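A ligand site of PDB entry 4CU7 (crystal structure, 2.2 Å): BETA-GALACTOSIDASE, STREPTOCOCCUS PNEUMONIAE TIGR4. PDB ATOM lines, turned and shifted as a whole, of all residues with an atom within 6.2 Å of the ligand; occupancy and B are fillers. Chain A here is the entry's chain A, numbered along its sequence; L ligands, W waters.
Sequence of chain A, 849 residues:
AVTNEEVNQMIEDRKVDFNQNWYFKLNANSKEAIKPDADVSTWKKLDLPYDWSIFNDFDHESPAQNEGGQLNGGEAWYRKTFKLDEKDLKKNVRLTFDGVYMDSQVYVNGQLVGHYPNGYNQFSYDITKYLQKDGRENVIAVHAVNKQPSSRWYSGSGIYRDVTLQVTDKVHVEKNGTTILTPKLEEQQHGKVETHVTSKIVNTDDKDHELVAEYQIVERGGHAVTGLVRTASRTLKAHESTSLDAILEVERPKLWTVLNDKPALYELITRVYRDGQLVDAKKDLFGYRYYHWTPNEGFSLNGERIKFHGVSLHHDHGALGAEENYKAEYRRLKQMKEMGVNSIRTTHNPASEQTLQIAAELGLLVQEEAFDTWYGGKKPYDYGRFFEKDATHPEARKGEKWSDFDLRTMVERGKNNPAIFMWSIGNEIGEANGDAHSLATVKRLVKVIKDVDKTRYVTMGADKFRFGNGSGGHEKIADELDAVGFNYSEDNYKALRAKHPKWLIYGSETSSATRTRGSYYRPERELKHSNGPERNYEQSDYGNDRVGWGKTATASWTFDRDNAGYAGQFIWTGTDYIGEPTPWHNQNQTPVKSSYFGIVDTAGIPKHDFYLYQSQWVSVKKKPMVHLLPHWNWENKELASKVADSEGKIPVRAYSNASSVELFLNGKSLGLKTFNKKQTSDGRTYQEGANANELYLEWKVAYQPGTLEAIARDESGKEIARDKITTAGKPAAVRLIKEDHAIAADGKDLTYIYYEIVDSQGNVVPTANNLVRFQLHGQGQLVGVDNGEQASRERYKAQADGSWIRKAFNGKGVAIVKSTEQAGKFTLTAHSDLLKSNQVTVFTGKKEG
Merely in contact with the ligand: Trp 572 (3.3 Å), Phe 597 (3.6 Å), Tyr 488 (3.8 Å) and Asn 427 (3.9 Å).
Hydrophobic or aromatic side chains within 4 Å of the ligand: His 348, Tyr 488, Trp 549, Trp 572 and Phe 597.
Within 4 Å of the ligand: Arg 152, His 348, Asn 427, Glu 428, Tyr 488, Glu 509, Ser 512, Trp 549, Trp 572, Glu 580 and Phe 597.
OE2 of Glu 580 is in hydrogen-bond range of O2 of the ligand.
A ring nitrogen (NE2) of His 348 is in hydrogen-bond range of an oxygen (O3) of the ligand.
OE2 of Glu 509 lies within salt-bridge range of N1 of the ligand, 2.7 Å away.
O1 of the ligand lies within hydrogen-bond range of OG of Ser 512 (2.7 Å).
An oxygen (O1) of the ligand is in hydrogen-bond range of the indole nitrogen (NE1) of Trp 549, at 2.9 Å.
The guanidinium group of Arg 152 is in hydrogen-bond range of an oxygen (O3) of the ligand (2.9 Å).
N1 of the ligand lies within salt-bridge range of OE2 of Glu 428.
Water W2 lies within hydrogen-bond range of NE2 of His 314, OE1 of Glu 580 and O3 of the ligand.
The side-chain carboxylate of Glu 580 lies within hydrogen-bond range of the side-chain hydroxyl of Tyr 577 (2.6 Å).
OE1 of Glu 509 is in hydrogen-bond range of ND2 of Asn 487 (3.4 Å).
The backbone carbonyl oxygen (O) of Trp 572 sits at hydrogen-bond distance from the backbone NH (N) of Ser 512, at 3.3 Å.
N of Val 547 sits at hydrogen-bond distance from O of Ser 512.
OD1 of Asp 372 is in salt-bridge range of NH2 of Arg 152.
The side-chain carboxylate (OE2) of Glu 428 is in hydrogen-bond range of the side-chain amide nitrogen (ND2) of Asn 487 (2.9 Å).
The indole nitrogen (NE1) of Trp 572 lies within hydrogen-bond range of the side-chain hydroxyl (OH) of Tyr 577, 3.1 Å away.
The side-chain amide oxygen (OD1) of Asn 427 lies within hydrogen-bond range of the side-chain amide nitrogen (ND2) of Asn 487.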
ATOM      1  N   ARG A 152      23.671  15.648 -14.934  1.00  0.00           N
ATOM      2  CA  ARG A 152      23.547  16.632 -13.854  1.00  0.00           C
ATOM      3  C   ARG A 152      22.134  16.608 -13.235  1.00  0.00           C
ATOM      4  O   ARG A 152      21.802  17.445 -12.403  1.00  0.00           O
ATOM      5  CB  ARG A 152      23.889  18.045 -14.352  1.00  0.00           C
ATOM      6  CG  ARG A 152      25.297  18.202 -14.974  1.00  0.00           C
ATOM      7  CD  ARG A 152      25.587  19.637 -15.424  1.00  0.00           C
ATOM      8  NE  ARG A 152      24.589  20.130 -16.384  1.00  0.00           N
ATOM      9  CZ  ARG A 152      23.578  20.922 -16.074  1.00  0.00           C
ATOM     10  NH1 ARG A 152      23.384  21.320 -14.820  1.00  0.00           N
ATOM     11  NH2 ARG A 152      22.728  21.341 -17.023  1.00  0.00           N
ATOM     12  N   TRP A 153      21.322  15.669 -13.690  1.00  0.00           N
ATOM     13  CA  TRP A 153      19.924  15.504 -13.206  1.00  0.00           C
ATOM     14  C   TRP A 153      19.612  14.032 -13.300  1.00  0.00           C
ATOM     15  O   TRP A 153      20.360  13.296 -13.899  1.00  0.00           O
ATOM     16  CB  TRP A 153      18.949  16.309 -14.092  1.00  0.00           C
ATOM     17  CG  TRP A 153      18.972  15.945 -15.573  1.00  0.00           C
ATOM     18  CD1 TRP A 153      18.218  14.973 -16.206  1.00  0.00           C
ATOM     19  CD2 TRP A 153      19.781  16.560 -16.578  1.00  0.00           C
ATOM     20  NE1 TRP A 153      18.512  14.961 -17.568  1.00  0.00           N
ATOM     21  CE2 TRP A 153      19.458  15.928 -17.814  1.00  0.00           C
ATOM     22  CE3 TRP A 153      20.708  17.612 -16.556  1.00  0.00           C
ATOM     23  CZ2 TRP A 153      20.066  16.294 -19.031  1.00  0.00           C
ATOM     24  CZ3 TRP A 153      21.312  17.973 -17.766  1.00  0.00           C
ATOM     25  CH2 TRP A 153      20.973  17.309 -18.991  1.00  0.00           C
ATOM     26  N   HIS A 314      12.485  19.161 -17.249  1.00  0.00           N
ATOM     27  CA  HIS A 314      13.225  17.907 -17.385  1.00  0.00           C
ATOM     28  C   HIS A 314      12.243  16.815 -17.752  1.00  0.00           C
ATOM     29  O   HIS A 314      11.023  17.003 -17.671  1.00  0.00           O
ATOM     30  CB  HIS A 314      14.002  17.586 -16.076  1.00  0.00           C
ATOM     31  CG  HIS A 314      15.387  18.158 -16.067  1.00  0.00           C
ATOM     32  ND1 HIS A 314      16.297  17.895 -17.072  1.00  0.00           N
ATOM     33  CD2 HIS A 314      16.039  18.961 -15.178  1.00  0.00           C
ATOM     34  CE1 HIS A 314      17.441  18.525 -16.829  1.00  0.00           C
ATOM     35  NE2 HIS A 314      17.310  19.179 -15.687  1.00  0.00           N
ATOM     36  N   THR A 347      14.784  21.119 -21.541  1.00  0.00           N
ATOM     37  CA  THR A 347      16.121  21.245 -20.947  1.00  0.00           C
ATOM     38  C   THR A 347      16.589  19.853 -20.455  1.00  0.00           C
ATOM     39  O   THR A 347      15.896  19.221 -19.652  1.00  0.00           O
ATOM     40  CB  THR A 347      16.042  22.223 -19.744  1.00  0.00           C
ATOM     41  OG1 THR A 347      14.953  21.828 -18.893  1.00  0.00           O
ATOM     42  CG2 THR A 347      15.796  23.642 -20.201  1.00  0.00           C
ATOM     43  N   HIS A 348      17.701  19.330 -20.964  1.00  0.00           N
ATOM     44  CA  HIS A 348      18.528  19.949 -22.021  1.00  0.00           C
ATOM     45  C   HIS A 348      18.815  18.822 -22.992  1.00  0.00           C
ATOM     46  O   HIS A 348      19.936  18.295 -23.052  1.00  0.00           O
ATOM     47  CB  HIS A 348      19.849  20.508 -21.456  1.00  0.00           C
ATOM     48  CG  HIS A 348      19.689  21.433 -20.288  1.00  0.00           C
ATOM     49  ND1 HIS A 348      19.257  22.735 -20.430  1.00  0.00           N
ATOM     50  CD2 HIS A 348      19.840  21.228 -18.961  1.00  0.00           C
ATOM     51  CE1 HIS A 348      19.196  23.311 -19.243  1.00  0.00           C
ATOM     52  NE2 HIS A 348      19.525  22.411 -18.330  1.00  0.00           N
ATOM     53  N   ASP A 372      23.548  19.459 -23.825  1.00  0.00           N
ATOM     54  CA  ASP A 372      23.985  20.011 -22.560  1.00  0.00           C
ATOM     55  C   ASP A 372      25.505  20.227 -22.515  1.00  0.00           C
ATOM     56  O   ASP A 372      26.021  20.855 -21.596  1.00  0.00           O
ATOM     57  CB  ASP A 372      23.562  19.105 -21.397  1.00  0.00           C
ATOM     58  CG  ASP A 372      23.784  19.777 -20.028  1.00  0.00           C
ATOM     59  OD1 ASP A 372      23.368  20.943 -19.805  1.00  0.00           O
ATOM     60  OD2 ASP A 372      24.362  19.118 -19.147  1.00  0.00           O
ATOM     61  N   ASN A 427      23.129  24.315 -23.994  1.00  0.00           N
ATOM     62  CA  ASN A 427      22.878  24.962 -22.704  1.00  0.00           C
ATOM     63  C   ASN A 427      24.174  25.104 -21.856  1.00  0.00           C
ATOM     64  O   ASN A 427      24.881  24.116 -21.577  1.00  0.00           O
ATOM     65  CB  ASN A 427      21.874  24.152 -21.904  1.00  0.00           C
ATOM     66  CG  ASN A 427      21.795  24.603 -20.455  1.00  0.00           C
ATOM     67  OD1 ASN A 427      21.305  25.705 -20.156  1.00  0.00           O
ATOM     68  ND2 ASN A 427      22.337  23.769 -19.555  1.00  0.00           N
ATOM     69  N   GLU A 428      24.448  26.349 -21.455  1.00  0.00           N
ATOM     70  CA  GLU A 428      25.586  26.709 -20.593  1.00  0.00           C
ATOM     71  C   GLU A 428      26.849  25.947 -21.042  1.00  0.00           C
ATOM     72  O   GLU A 428      27.451  25.189 -20.256  1.00  0.00           O
ATOM     73  CB  GLU A 428      25.257  26.458 -19.107  1.00  0.00           C
ATOM     74  CG  GLU A 428      24.068  27.295 -18.652  1.00  0.00           C
ATOM     75  CD  GLU A 428      23.748  27.195 -17.176  1.00  0.00           C
ATOM     76  OE1 GLU A 428      24.238  26.274 -16.481  1.00  0.00           O
ATOM     77  OE2 GLU A 428      22.953  28.025 -16.702  1.00  0.00           O
ATOM     78  N   ASN A 487      20.863  33.136 -19.721  1.00  0.00           N
ATOM     79  CA  ASN A 487      20.586  32.426 -18.469  1.00  0.00           C
ATOM     80  C   ASN A 487      20.970  33.305 -17.300  1.00  0.00           C
ATOM     81  O   ASN A 487      22.151  33.622 -17.114  1.00  0.00           O
ATOM     82  CB  ASN A 487      21.382  31.106 -18.356  1.00  0.00           C
ATOM     83  CG  ASN A 487      20.826  29.985 -19.222  1.00  0.00           C
ATOM     84  OD1 ASN A 487      20.106  30.201 -20.241  1.00  0.00           O
ATOM     85  ND2 ASN A 487      21.156  28.738 -18.825  1.00  0.00           N
ATOM     86  N   TYR A 488      19.971  33.660 -16.469  1.00  0.00           N
ATOM     87  CA  TYR A 488      20.208  34.414 -15.235  1.00  0.00           C
ATOM     88  C   TYR A 488      20.973  35.724 -15.435  1.00  0.00           C
ATOM     89  O   TYR A 488      21.731  36.137 -14.558  1.00  0.00           O
ATOM     90  CB  TYR A 488      20.876  33.539 -14.150  1.00  0.00           C
ATOM     91  CG  TYR A 488      20.182  32.195 -14.008  1.00  0.00           C
ATOM     92  CD1 TYR A 488      18.992  32.061 -13.266  1.00  0.00           C
ATOM     93  CD2 TYR A 488      20.669  31.089 -14.705  1.00  0.00           C
ATOM     94  CE1 TYR A 488      18.326  30.838 -13.206  1.00  0.00           C
ATOM     95  CE2 TYR A 488      20.006  29.857 -14.649  1.00  0.00           C
ATOM     96  CZ  TYR A 488      18.844  29.738 -13.896  1.00  0.00           C
ATOM     97  OH  TYR A 488      18.200  28.520 -13.834  1.00  0.00           O
ATOM     98  N   GLU A 509      16.853  30.974 -19.517  1.00  0.00           N
ATOM     99  CA  GLU A 509      16.686  30.309 -18.218  1.00  0.00           C
ATOM    100  C   GLU A 509      16.686  31.298 -17.093  1.00  0.00           C
ATOM    101  O   GLU A 509      17.603  32.127 -16.975  1.00  0.00           O
ATOM    102  CB  GLU A 509      17.794  29.304 -17.973  1.00  0.00           C
ATOM    103  CG  GLU A 509      17.288  27.999 -17.338  1.00  0.00           C
ATOM    104  CD  GLU A 509      18.435  27.055 -17.024  1.00  0.00           C
ATOM    105  OE1 GLU A 509      18.898  26.356 -17.935  1.00  0.00           O
ATOM    106  OE2 GLU A 509      18.878  27.059 -15.864  1.00  0.00           O
ATOM    107  N   SER A 511      15.219  32.460 -12.810  1.00  0.00           N
ATOM    108  CA  SER A 511      14.696  32.382 -11.445  1.00  0.00           C
ATOM    109  C   SER A 511      15.518  31.373 -10.658  1.00  0.00           C
ATOM    110  O   SER A 511      16.607  31.651 -10.226  1.00  0.00           O
ATOM    111  CB  SER A 511      13.209  32.022 -11.414  1.00  0.00           C
ATOM    112  OG  SER A 511      12.718  32.110 -10.078  1.00  0.00           O
ATOM    113  N   SER A 512      15.231  30.062 -10.747  1.00  0.00           N
ATOM    114  CA  SER A 512      15.871  29.088  -9.848  1.00  0.00           C
ATOM    115  C   SER A 512      15.627  29.483  -8.405  1.00  0.00           C
ATOM    116  O   SER A 512      16.507  29.328  -7.532  1.00  0.00           O
ATOM    117  CB  SER A 512      17.372  28.902 -10.118  1.00  0.00           C
ATOM    118  OG  SER A 512      17.613  27.920 -11.121  1.00  0.00           O
ATOM    119  N   VAL A 547      18.645  30.574  -5.227  1.00  0.00           N
ATOM    120  CA  VAL A 547      20.037  30.210  -5.251  1.00  0.00           C
ATOM    121  C   VAL A 547      20.940  31.431  -5.464  1.00  0.00           C
ATOM    122  O   VAL A 547      20.459  32.507  -5.825  1.00  0.00           O
ATOM    123  CB  VAL A 547      20.328  29.113  -6.292  1.00  0.00           C
ATOM    124  CG1 VAL A 547      19.577  27.834  -5.915  1.00  0.00           C
ATOM    125  CG2 VAL A 547      20.001  29.573  -7.735  1.00  0.00           C
ATOM    126  N   TRP A 549      22.931  32.383  -7.760  1.00  0.00           N
ATOM    127  CA  TRP A 549      22.851  32.984  -9.103  1.00  0.00           C
ATOM    128  C   TRP A 549      21.419  33.297  -9.550  1.00  0.00           C
ATOM    129  O   TRP A 549      21.206  33.746 -10.670  1.00  0.00           O
ATOM    130  CB  TRP A 549      23.509  32.058 -10.115  1.00  0.00           C
ATOM    131  CG  TRP A 549      22.929  30.658 -10.109  1.00  0.00           C
ATOM    132  CD1 TRP A 549      21.934  30.179 -10.909  1.00  0.00           C
ATOM    133  CD2 TRP A 549      23.336  29.566  -9.275  1.00  0.00           C
ATOM    134  NE1 TRP A 549      21.691  28.863 -10.633  1.00  0.00           N
ATOM    135  CE2 TRP A 549      22.550  28.450  -9.639  1.00  0.00           C
ATOM    136  CE3 TRP A 549      24.304  29.422  -8.233  1.00  0.00           C
ATOM    137  CZ2 TRP A 549      22.667  27.192  -9.008  1.00  0.00           C
ATOM    138  CZ3 TRP A 549      24.448  28.151  -7.608  1.00  0.00           C
ATOM    139  CH2 TRP A 549      23.620  27.055  -8.021  1.00  0.00           C
ATOM    140  N   TRP A 572      13.281  28.143 -14.594  1.00  0.00           N
ATOM    141  CA  TRP A 572      13.840  26.932 -14.015  1.00  0.00           C
ATOM    142  C   TRP A 572      13.173  26.673 -12.665  1.00  0.00           C
ATOM    143  O   TRP A 572      13.514  27.373 -11.687  1.00  0.00           O
ATOM    144  CB  TRP A 572      15.382  27.106 -13.803  1.00  0.00           C
ATOM    145  CG  TRP A 572      16.015  25.787 -13.588  1.00  0.00           C
ATOM    146  CD1 TRP A 572      16.321  25.205 -12.379  1.00  0.00           C
ATOM    147  CD2 TRP A 572      16.319  24.816 -14.600  1.00  0.00           C
ATOM    148  NE1 TRP A 572      16.812  23.953 -12.585  1.00  0.00           N
ATOM    149  CE2 TRP A 572      16.811  23.671 -13.930  1.00  0.00           C
ATOM    150  CE3 TRP A 572      16.203  24.797 -16.011  1.00  0.00           C
ATOM    151  CZ2 TRP A 572      17.186  22.526 -14.609  1.00  0.00           C
ATOM    152  CZ3 TRP A 572      16.586  23.639 -16.680  1.00  0.00           C
ATOM    153  CH2 TRP A 572      17.076  22.530 -15.990  1.00  0.00           C
ATOM    154  N   TYR A 577      12.003  17.896 -10.403  1.00  0.00           N
ATOM    155  CA  TYR A 577      12.492  16.679 -11.074  1.00  0.00           C
ATOM    156  C   TYR A 577      13.404  15.959 -10.086  1.00  0.00           C
ATOM    157  O   TYR A 577      13.872  16.570  -9.101  1.00  0.00           O
ATOM    158  CB  TYR A 577      13.270  17.073 -12.349  1.00  0.00           C
ATOM    159  CG  TYR A 577      14.339  18.143 -12.112  1.00  0.00           C
ATOM    160  CD1 TYR A 577      13.997  19.488 -12.053  1.00  0.00           C
ATOM    161  CD2 TYR A 577      15.708  17.781 -11.995  1.00  0.00           C
ATOM    162  CE1 TYR A 577      14.956  20.460 -11.818  1.00  0.00           C
ATOM    163  CE2 TYR A 577      16.687  18.749 -11.815  1.00  0.00           C
ATOM    164  CZ  TYR A 577      16.297  20.083 -11.712  1.00  0.00           C
ATOM    165  OH  TYR A 577      17.245  21.059 -11.518  1.00  0.00           O
ATOM    166  N   GLU A 580      19.415  16.926  -8.726  1.00  0.00           N
ATOM    167  CA  GLU A 580      19.788  18.324  -8.490  1.00  0.00           C
ATOM    168  C   GLU A 580      19.124  19.020  -7.307  1.00  0.00           C
ATOM    169  O   GLU A 580      18.398  19.987  -7.493  1.00  0.00           O
ATOM    170  CB  GLU A 580      19.699  19.131  -9.796  1.00  0.00           C
ATOM    171  CG  GLU A 580      20.523  20.417  -9.735  1.00  0.00           C
ATOM    172  CD  GLU A 580      20.619  21.124 -11.074  1.00  0.00           C
ATOM    173  OE1 GLU A 580      19.754  20.885 -11.960  1.00  0.00           O
ATOM    174  OE2 GLU A 580      21.565  21.949 -11.248  1.00  0.00           O
ATOM    175  N   THR A 582      19.833  21.266  -5.131  1.00  0.00           N
ATOM    176  CA  THR A 582      20.335  22.564  -4.729  1.00  0.00           C
ATOM    177  C   THR A 582      19.246  23.277  -3.933  1.00  0.00           C
ATOM    178  O   THR A 582      18.105  23.284  -4.358  1.00  0.00           O
ATOM    179  CB  THR A 582      20.663  23.353  -5.997  1.00  0.00           C
ATOM    180  OG1 THR A 582      21.431  22.487  -6.863  1.00  0.00           O
ATOM    181  CG2 THR A 582      21.445  24.655  -5.682  1.00  0.00           C
ATOM    182  N   PHE A 597      13.453  23.487  -7.330  1.00  0.00           N
ATOM    183  CA  PHE A 597      13.252  24.569  -8.323  1.00  0.00           C
ATOM    184  C   PHE A 597      11.858  24.675  -8.919  1.00  0.00           C
ATOM    185  O   PHE A 597      11.494  25.711  -9.480  1.00  0.00           O
ATOM    186  CB  PHE A 597      14.200  24.381  -9.482  1.00  0.00           C
ATOM    187  CG  PHE A 597      15.681  24.462  -9.115  1.00  0.00           C
ATOM    188  CD1 PHE A 597      16.228  25.626  -8.599  1.00  0.00           C
ATOM    189  CD2 PHE A 597      16.514  23.405  -9.393  1.00  0.00           C
ATOM    190  CE1 PHE A 597      17.589  25.723  -8.326  1.00  0.00           C
ATOM    191  CE2 PHE A 597      17.886  23.494  -9.118  1.00  0.00           C
ATOM    192  CZ  PHE A 597      18.410  24.630  -8.580  1.00  0.00           C
HETATM  193  C1  LIG L   1      21.324  24.854 -15.959  1.00  0.00           C
HETATM  194  N1  LIG L   1      21.299  26.147 -15.261  1.00  0.00           N
HETATM  195  O1  LIG L   1      20.020  26.597 -11.103  1.00  0.00           O
HETATM  196  C2  LIG L   1      20.273  23.922 -15.330  1.00  0.00           C
HETATM  197  O2  LIG L   1      21.633  23.292 -13.360  1.00  0.00           O
HETATM  198  C3  LIG L   1      20.375  23.872 -13.789  1.00  0.00           C
HETATM  199  O3  LIG L   1      20.400  22.617 -15.904  1.00  0.00           O
HETATM  200  C4  LIG L   1      20.212  25.269 -13.221  1.00  0.00           C
HETATM  201  C5  LIG L   1      21.325  26.150 -13.793  1.00  0.00           C
HETATM  202  C6  LIG L   1      20.198  25.277 -11.683  1.00  0.00           C
HETATM  203  O   HOH W   1      24.312  24.009 -12.158  1.00  0.00           O
HETATM  204  O   HOH W   2      19.593  20.280 -14.633  1.00  0.00           O
